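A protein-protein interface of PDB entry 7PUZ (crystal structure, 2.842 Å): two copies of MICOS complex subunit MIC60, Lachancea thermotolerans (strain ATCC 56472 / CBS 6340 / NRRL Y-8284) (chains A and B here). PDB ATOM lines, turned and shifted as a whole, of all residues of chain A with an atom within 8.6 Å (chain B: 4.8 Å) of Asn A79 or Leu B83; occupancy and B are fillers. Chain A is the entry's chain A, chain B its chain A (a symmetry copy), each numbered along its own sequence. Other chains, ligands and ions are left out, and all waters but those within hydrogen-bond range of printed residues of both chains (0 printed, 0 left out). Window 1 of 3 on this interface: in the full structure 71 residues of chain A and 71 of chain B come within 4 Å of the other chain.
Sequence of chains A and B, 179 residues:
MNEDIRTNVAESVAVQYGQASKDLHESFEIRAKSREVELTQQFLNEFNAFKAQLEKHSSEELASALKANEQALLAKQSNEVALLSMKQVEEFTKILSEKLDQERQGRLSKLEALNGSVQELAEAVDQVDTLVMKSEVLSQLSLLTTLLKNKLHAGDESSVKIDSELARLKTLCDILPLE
The side-chain amide nitrogen of Asn A79 is in hydrogen-bond range of the backbone carbonyl oxygen of Ala B82.
The backbone carbonyl oxygen of Ala A82 sits at hydrogen-bond distance from the side-chain amide nitrogen of Asn B79 (3.3 Å).
Among the printed residues, merely in contact across the chains: Met A86 with Asn B79, Asn A79 with Met B86, Leu A83 with Glu B80, Glu A80 with Leu B83, Asn A79 with Leu B83, Leu A83 with Asn B79, Lys A76 with Leu B83, Ala A75 with Met B86 and Lys A76 with Met B86.
Gln A77 touches none of the printed residues of chain B.
Asn A79 touches just these residues of chain B: Ala B82 (3.3 Å), Leu B83 (3.7 Å) and Met B86 (3.4 Å).
Printed residues of chain B within 4 Å of Ala A82: Asn B79 (3.3 Å).
Of the printed residues of chain A, Glu B80 touches Leu A83.
Val B81 touches none of the printed residues of chain A.
Of chain A, only Asn A79 comes within 4 Å of Ala B82.
Leu B83 touches three residues of chain A.
The nearest residue of chain B that does not touch Asn A79 is Asn B79 (4.4 Å).
The nearest residue of chain A that does not touch Leu B83 is Leu A83 (5.9 Å).
The nearest printed residue of chain B that does not touch Lys A76 is Lys B87 (4.4 Å).
Of the 9 printed residues of chain B, 5 touch a printed residue of chain A.
Hydrophobic or aromatic side chains of chain B that line the printed part of chain A: Ala B82, Leu B83 and Met B86.
Printed residues of chain A that touch a printed residue of chain B: Ala A75, Lys A76, Asn A79, Glu A80, Ala A82, Leu A83 and Met A86.
Hydrophobic or aromatic side chains of chain A within 4 Å of the printed part of chain B: Ala A75, Ala A82, Leu A83 and Met A86.
Asn A79 touches Ala B82, and with the chains exchanged Ala A82 touches Asn B79.
Asn A79 touches Leu B83, and with the chains exchanged Leu A83 touches Asn B79.
Asn A79 touches Met B86, and with the chains exchanged Met A86 touches Asn B79.
Glu A80 touches Leu B83, and with the chains exchanged Leu A83 touches Glu B80.
8 positions are printed for both chains.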
ATOM      1  N   GLN A  71     -13.462 -14.694  21.086  1.00  0.00           N
ATOM      2  CA  GLN A  71     -14.309 -13.951  20.159  1.00  0.00           C
ATOM      3  C   GLN A  71     -13.568 -13.639  18.865  1.00  0.00           C
ATOM      4  O   GLN A  71     -14.146 -13.735  17.776  1.00  0.00           O
ATOM      5  CB  GLN A  71     -14.812 -12.669  20.818  1.00  0.00           C
ATOM      6  CG  GLN A  71     -15.648 -12.911  22.066  1.00  0.00           C
ATOM      7  CD  GLN A  71     -16.926 -13.680  21.781  1.00  0.00           C
ATOM      8  OE1 GLN A  71     -17.213 -14.693  22.424  1.00  0.00           O
ATOM      9  NE2 GLN A  71     -17.709 -13.197  20.820  1.00  0.00           N
ATOM     10  N   ALA A  72     -12.285 -13.276  18.961  1.00  0.00           N
ATOM     11  CA  ALA A  72     -11.494 -13.055  17.755  1.00  0.00           C
ATOM     12  C   ALA A  72     -11.363 -14.335  16.940  1.00  0.00           C
ATOM     13  O   ALA A  72     -11.416 -14.303  15.704  1.00  0.00           O
ATOM     14  CB  ALA A  72     -10.116 -12.510  18.121  1.00  0.00           C
ATOM     15  N   LEU A  73     -11.202 -15.475  17.616  1.00  0.00           N
ATOM     16  CA  LEU A  73     -11.108 -16.747  16.908  1.00  0.00           C
ATOM     17  C   LEU A  73     -12.421 -17.092  16.212  1.00  0.00           C
ATOM     18  O   LEU A  73     -12.419 -17.553  15.062  1.00  0.00           O
ATOM     19  CB  LEU A  73     -10.703 -17.855  17.880  1.00  0.00           C
ATOM     20  CG  LEU A  73     -10.480 -19.235  17.261  1.00  0.00           C
ATOM     21  CD1 LEU A  73      -9.427 -19.173  16.158  1.00  0.00           C
ATOM     22  CD2 LEU A  73     -10.084 -20.237  18.328  1.00  0.00           C
ATOM     23  N   LEU A  74     -13.549 -16.881  16.896  1.00  0.00           N
ATOM     24  CA  LEU A  74     -14.847 -17.101  16.267  1.00  0.00           C
ATOM     25  C   LEU A  74     -15.030 -16.193  15.059  1.00  0.00           C
ATOM     26  O   LEU A  74     -15.558 -16.624  14.027  1.00  0.00           O
ATOM     27  CB  LEU A  74     -15.973 -16.875  17.277  1.00  0.00           C
ATOM     28  CG  LEU A  74     -17.390 -17.022  16.708  1.00  0.00           C
ATOM     29  CD1 LEU A  74     -17.608 -18.422  16.164  1.00  0.00           C
ATOM     30  CD2 LEU A  74     -18.442 -16.687  17.756  1.00  0.00           C
ATOM     31  N   ALA A  75     -14.591 -14.936  15.164  1.00  0.00           N
ATOM     32  CA  ALA A  75     -14.721 -14.011  14.041  1.00  0.00           C
ATOM     33  C   ALA A  75     -13.861 -14.445  12.859  1.00  0.00           C
ATOM     34  O   ALA A  75     -14.297 -14.363  11.705  1.00  0.00           O
ATOM     35  CB  ALA A  75     -14.353 -12.598  14.483  1.00  0.00           C
ATOM     36  N   LYS A  76     -12.639 -14.913  13.127  1.00  0.00           N
ATOM     37  CA  LYS A  76     -11.778 -15.391  12.047  1.00  0.00           C
ATOM     38  C   LYS A  76     -12.376 -16.617  11.362  1.00  0.00           C
ATOM     39  O   LYS A  76     -12.361 -16.717  10.126  1.00  0.00           O
ATOM     40  CB  LYS A  76     -10.383 -15.702  12.584  1.00  0.00           C
ATOM     41  CG  LYS A  76      -9.506 -16.471  11.608  1.00  0.00           C
ATOM     42  CD  LYS A  76      -8.063 -16.528  12.081  1.00  0.00           C
ATOM     43  CE  LYS A  76      -7.505 -17.942  12.004  1.00  0.00           C
ATOM     44  NZ  LYS A  76      -7.955 -18.782  13.156  1.00  0.00           N
ATOM     45  N   GLN A  77     -12.910 -17.559  12.144  1.00  0.00           N
ATOM     46  CA  GLN A  77     -13.524 -18.739  11.544  1.00  0.00           C
ATOM     47  C   GLN A  77     -14.780 -18.372  10.758  1.00  0.00           C
ATOM     48  O   GLN A  77     -15.059 -18.960   9.703  1.00  0.00           O
ATOM     49  CB  GLN A  77     -13.831 -19.774  12.626  1.00  0.00           C
ATOM     50  CG  GLN A  77     -12.583 -20.406  13.218  1.00  0.00           C
ATOM     51  CD  GLN A  77     -12.887 -21.356  14.360  1.00  0.00           C
ATOM     52  OE1 GLN A  77     -13.349 -20.939  15.422  1.00  0.00           O
ATOM     53  NE2 GLN A  77     -12.632 -22.642  14.143  1.00  0.00           N
ATOM     54  N   SER A  78     -15.543 -17.392  11.250  1.00  0.00           N
ATOM     55  CA  SER A  78     -16.692 -16.894  10.499  1.00  0.00           C
ATOM     56  C   SER A  78     -16.253 -16.297   9.170  1.00  0.00           C
ATOM     57  O   SER A  78     -16.887 -16.526   8.134  1.00  0.00           O
ATOM     58  CB  SER A  78     -17.450 -15.854  11.326  1.00  0.00           C
ATOM     59  OG  SER A  78     -17.986 -16.428  12.504  1.00  0.00           O
ATOM     60  N   ASN A  79     -15.168 -15.519   9.186  1.00  0.00           N
ATOM     61  CA  ASN A  79     -14.654 -14.944   7.949  1.00  0.00           C
ATOM     62  C   ASN A  79     -14.226 -16.031   6.973  1.00  0.00           C
ATOM     63  O   ASN A  79     -14.452 -15.912   5.766  1.00  0.00           O
ATOM     64  CB  ASN A  79     -13.489 -14.001   8.243  1.00  0.00           C
ATOM     65  CG  ASN A  79     -13.937 -12.699   8.877  1.00  0.00           C
ATOM     66  OD1 ASN A  79     -15.113 -12.336   8.814  1.00  0.00           O
ATOM     67  ND2 ASN A  79     -12.997 -11.982   9.485  1.00  0.00           N
ATOM     68  N   GLU A  80     -13.609 -17.103   7.477  1.00  0.00           N
ATOM     69  CA  GLU A  80     -13.179 -18.185   6.592  1.00  0.00           C
ATOM     70  C   GLU A  80     -14.376 -18.889   5.955  1.00  0.00           C
ATOM     71  O   GLU A  80     -14.389 -19.154   4.742  1.00  0.00           O
ATOM     72  CB  GLU A  80     -12.308 -19.178   7.363  1.00  0.00           C
ATOM     73  CG  GLU A  80     -10.949 -18.626   7.753  1.00  0.00           C
ATOM     74  CD  GLU A  80     -10.212 -19.515   8.737  1.00  0.00           C
ATOM     75  OE1 GLU A  80     -10.726 -20.608   9.054  1.00  0.00           O
ATOM     76  OE2 GLU A  80      -9.120 -19.118   9.198  1.00  0.00           O
ATOM     77  N   VAL A  81     -15.394 -19.205   6.762  1.00  0.00           N
ATOM     78  CA  VAL A  81     -16.595 -19.845   6.227  1.00  0.00           C
ATOM     79  C   VAL A  81     -17.268 -18.945   5.194  1.00  0.00           C
ATOM     80  O   VAL A  81     -17.691 -19.405   4.119  1.00  0.00           O
ATOM     81  CB  VAL A  81     -17.558 -20.218   7.372  1.00  0.00           C
ATOM     82  CG1 VAL A  81     -18.928 -20.571   6.820  1.00  0.00           C
ATOM     83  CG2 VAL A  81     -16.999 -21.377   8.180  1.00  0.00           C
ATOM     84  N   ALA A  82     -17.369 -17.648   5.498  1.00  0.00           N
ATOM     85  CA  ALA A  82     -17.977 -16.711   4.559  1.00  0.00           C
ATOM     86  C   ALA A  82     -17.158 -16.603   3.278  1.00  0.00           C
ATOM     87  O   ALA A  82     -17.724 -16.484   2.191  1.00  0.00           O
ATOM     88  CB  ALA A  82     -18.138 -15.339   5.213  1.00  0.00           C
ATOM     89  N   LEU A  83     -15.829 -16.666   3.383  1.00  0.00           N
ATOM     90  CA  LEU A  83     -14.982 -16.588   2.197  1.00  0.00           C
ATOM     91  C   LEU A  83     -15.178 -17.808   1.302  1.00  0.00           C
ATOM     92  O   LEU A  83     -15.196 -17.687   0.070  1.00  0.00           O
ATOM     93  CB  LEU A  83     -13.519 -16.440   2.626  1.00  0.00           C
ATOM     94  CG  LEU A  83     -12.397 -16.150   1.622  1.00  0.00           C
ATOM     95  CD1 LEU A  83     -11.733 -17.437   1.148  1.00  0.00           C
ATOM     96  CD2 LEU A  83     -12.904 -15.331   0.442  1.00  0.00           C
ATOM     97  N   LEU A  84     -15.337 -18.989   1.902  1.00  0.00           N
ATOM     98  CA  LEU A  84     -15.620 -20.184   1.105  1.00  0.00           C
ATOM     99  C   LEU A  84     -16.971 -20.065   0.400  1.00  0.00           C
ATOM    100  O   LEU A  84     -17.072 -20.226  -0.831  1.00  0.00           O
ATOM    101  CB  LEU A  84     -15.576 -21.422   2.005  1.00  0.00           C
ATOM    102  CG  LEU A  84     -15.363 -22.810   1.398  1.00  0.00           C
ATOM    103  CD1 LEU A  84     -14.658 -23.714   2.404  1.00  0.00           C
ATOM    104  CD2 LEU A  84     -16.689 -23.426   0.947  1.00  0.00           C
ATOM    105  N   SER A  85     -18.026 -19.778   1.171  1.00  0.00           N
ATOM    106  CA  SER A  85     -19.347 -19.601   0.573  1.00  0.00           C
ATOM    107  C   SER A  85     -19.343 -18.496  -0.474  1.00  0.00           C
ATOM    108  O   SER A  85     -20.120 -18.546  -1.437  1.00  0.00           O
ATOM    109  CB  SER A  85     -20.384 -19.301   1.657  1.00  0.00           C
ATOM    110  OG  SER A  85     -20.618 -20.436   2.474  1.00  0.00           O
ATOM    111  N   MET A  86     -18.451 -17.514  -0.330  1.00  0.00           N
ATOM    112  CA  MET A  86     -18.416 -16.403  -1.265  1.00  0.00           C
ATOM    113  C   MET A  86     -17.661 -16.740  -2.536  1.00  0.00           C
ATOM    114  O   MET A  86     -18.026 -16.247  -3.601  1.00  0.00           O
ATOM    115  CB  MET A  86     -17.817 -15.172  -0.593  1.00  0.00           C
ATOM    116  CG  MET A  86     -18.859 -14.304   0.093  1.00  0.00           C
ATOM    117  SD  MET A  86     -20.192 -13.818  -1.026  1.00  0.00           S
ATOM    118  CE  MET A  86     -21.474 -15.010  -0.628  1.00  0.00           C
ATOM    119  N   ASN B  79     -14.563 -10.023   2.877  1.00  0.00           N
ATOM    120  CA  ASN B  79     -14.213 -11.183   3.687  1.00  0.00           C
ATOM    121  C   ASN B  79     -12.708 -11.409   3.704  1.00  0.00           C
ATOM    122  O   ASN B  79     -12.141 -11.759   4.743  1.00  0.00           O
ATOM    123  CB  ASN B  79     -14.934 -12.429   3.173  1.00  0.00           C
ATOM    124  CG  ASN B  79     -16.415 -12.422   3.494  1.00  0.00           C
ATOM    125  OD1 ASN B  79     -16.870 -11.678   4.365  1.00  0.00           O
ATOM    126  ND2 ASN B  79     -17.177 -13.260   2.798  1.00  0.00           N
ATOM    127  N   GLU B  80     -12.042 -11.208   2.565  1.00  0.00           N
ATOM    128  CA  GLU B  80     -10.593 -11.400   2.519  1.00  0.00           C
ATOM    129  C   GLU B  80      -9.869 -10.375   3.391  1.00  0.00           C
ATOM    130  O   GLU B  80      -8.956 -10.721   4.158  1.00  0.00           O
ATOM    131  CB  GLU B  80     -10.101 -11.333   1.073  1.00  0.00           C
ATOM    132  CG  GLU B  80     -10.532 -12.515   0.223  1.00  0.00           C
ATOM    133  CD  GLU B  80     -10.269 -12.304  -1.256  1.00  0.00           C
ATOM    134  OE1 GLU B  80      -9.672 -11.267  -1.614  1.00  0.00           O
ATOM    135  OE2 GLU B  80     -10.664 -13.174  -2.062  1.00  0.00           O
ATOM    136  N   VAL B  81     -10.262  -9.102   3.282  1.00  0.00           N
ATOM    137  CA  VAL B  81      -9.649  -8.063   4.109  1.00  0.00           C
ATOM    138  C   VAL B  81      -9.881  -8.348   5.590  1.00  0.00           C
ATOM    139  O   VAL B  81      -8.964  -8.225   6.420  1.00  0.00           O
ATOM    140  CB  VAL B  81     -10.183  -6.674   3.706  1.00  0.00           C
ATOM    141  CG1 VAL B  81      -9.817  -5.639   4.755  1.00  0.00           C
ATOM    142  CG2 VAL B  81      -9.634  -6.267   2.348  1.00  0.00           C
ATOM    143  N   ALA B  82     -11.107  -8.746   5.943  1.00  0.00           N
ATOM    144  CA  ALA B  82     -11.412  -9.063   7.334  1.00  0.00           C
ATOM    145  C   ALA B  82     -10.612 -10.269   7.814  1.00  0.00           C
ATOM    146  O   ALA B  82     -10.173 -10.302   8.964  1.00  0.00           O
ATOM    147  CB  ALA B  82     -12.910  -9.308   7.503  1.00  0.00           C
ATOM    148  N   LEU B  83     -10.395 -11.256   6.943  1.00  0.00           N
ATOM    149  CA  LEU B  83      -9.621 -12.434   7.326  1.00  0.00           C
ATOM    150  C   LEU B  83      -8.165 -12.069   7.597  1.00  0.00           C
ATOM    151  O   LEU B  83      -7.548 -12.595   8.533  1.00  0.00           O
ATOM    152  CB  LEU B  83      -9.736 -13.496   6.229  1.00  0.00           C
ATOM    153  CG  LEU B  83      -9.190 -14.918   6.407  1.00  0.00           C
ATOM    154  CD1 LEU B  83      -7.777 -15.041   5.852  1.00  0.00           C
ATOM    155  CD2 LEU B  83      -9.244 -15.357   7.865  1.00  0.00           C
ATOM    156  N   LEU B  84      -7.601 -11.163   6.796  1.00  0.00           N
ATOM    157  CA  LEU B  84      -6.236 -10.701   7.057  1.00  0.00           C
ATOM    158  C   LEU B  84      -6.155  -9.960   8.391  1.00  0.00           C
ATOM    159  O   LEU B  84      -5.329 -10.290   9.264  1.00  0.00           O
ATOM    160  CB  LEU B  84      -5.766  -9.812   5.903  1.00  0.00           C
ATOM    161  CG  LEU B  84      -4.273  -9.583   5.664  1.00  0.00           C
ATOM    162  CD1 LEU B  84      -4.017  -9.331   4.182  1.00  0.00           C
ATOM    163  CD2 LEU B  84      -3.750  -8.422   6.513  1.00  0.00           C
ATOM    164  N   SER B  85      -7.012  -8.948   8.567  1.00  0.00           N
ATOM    165  CA  SER B  85      -7.034  -8.214   9.830  1.00  0.00           C
ATOM    166  C   SER B  85      -7.304  -9.139  11.009  1.00  0.00           C
ATOM    167  O   SER B  85      -6.839  -8.877  12.127  1.00  0.00           O
ATOM    168  CB  SER B  85      -8.081  -7.100   9.779  1.00  0.00           C
ATOM    169  OG  SER B  85      -7.693  -6.069   8.885  1.00  0.00           O
ATOM    170  N   MET B  86      -8.015 -10.243  10.776  1.00  0.00           N
ATOM    171  CA  MET B  86      -8.350 -11.151  11.860  1.00  0.00           C
ATOM    172  C   MET B  86      -7.214 -12.097  12.193  1.00  0.00           C
ATOM    173  O   MET B  86      -7.050 -12.453  13.358  1.00  0.00           O
ATOM    174  CB  MET B  86      -9.616 -11.929  11.518  1.00  0.00           C
ATOM    175  CG  MET B  86     -10.885 -11.229  11.977  1.00  0.00           C
ATOM    176  SD  MET B  86     -10.851 -10.833  13.739  1.00  0.00           S
ATOM    177  CE  MET B  86     -10.355  -9.108  13.731  1.00  0.00           C
ATOM    178  N   LYS B  87      -6.421 -12.509  11.205  1.00  0.00           N
ATOM    179  CA  LYS B  87      -5.157 -13.161  11.529  1.00  0.00           C
ATOM    180  C   LYS B  87      -4.301 -12.255  12.408  1.00  0.00           C
ATOM    181  O   LYS B  87      -3.730 -12.702  13.415  1.00  0.00           O
ATOM    182  CB  LYS B  87      -4.411 -13.543  10.250  1.00  0.00           C
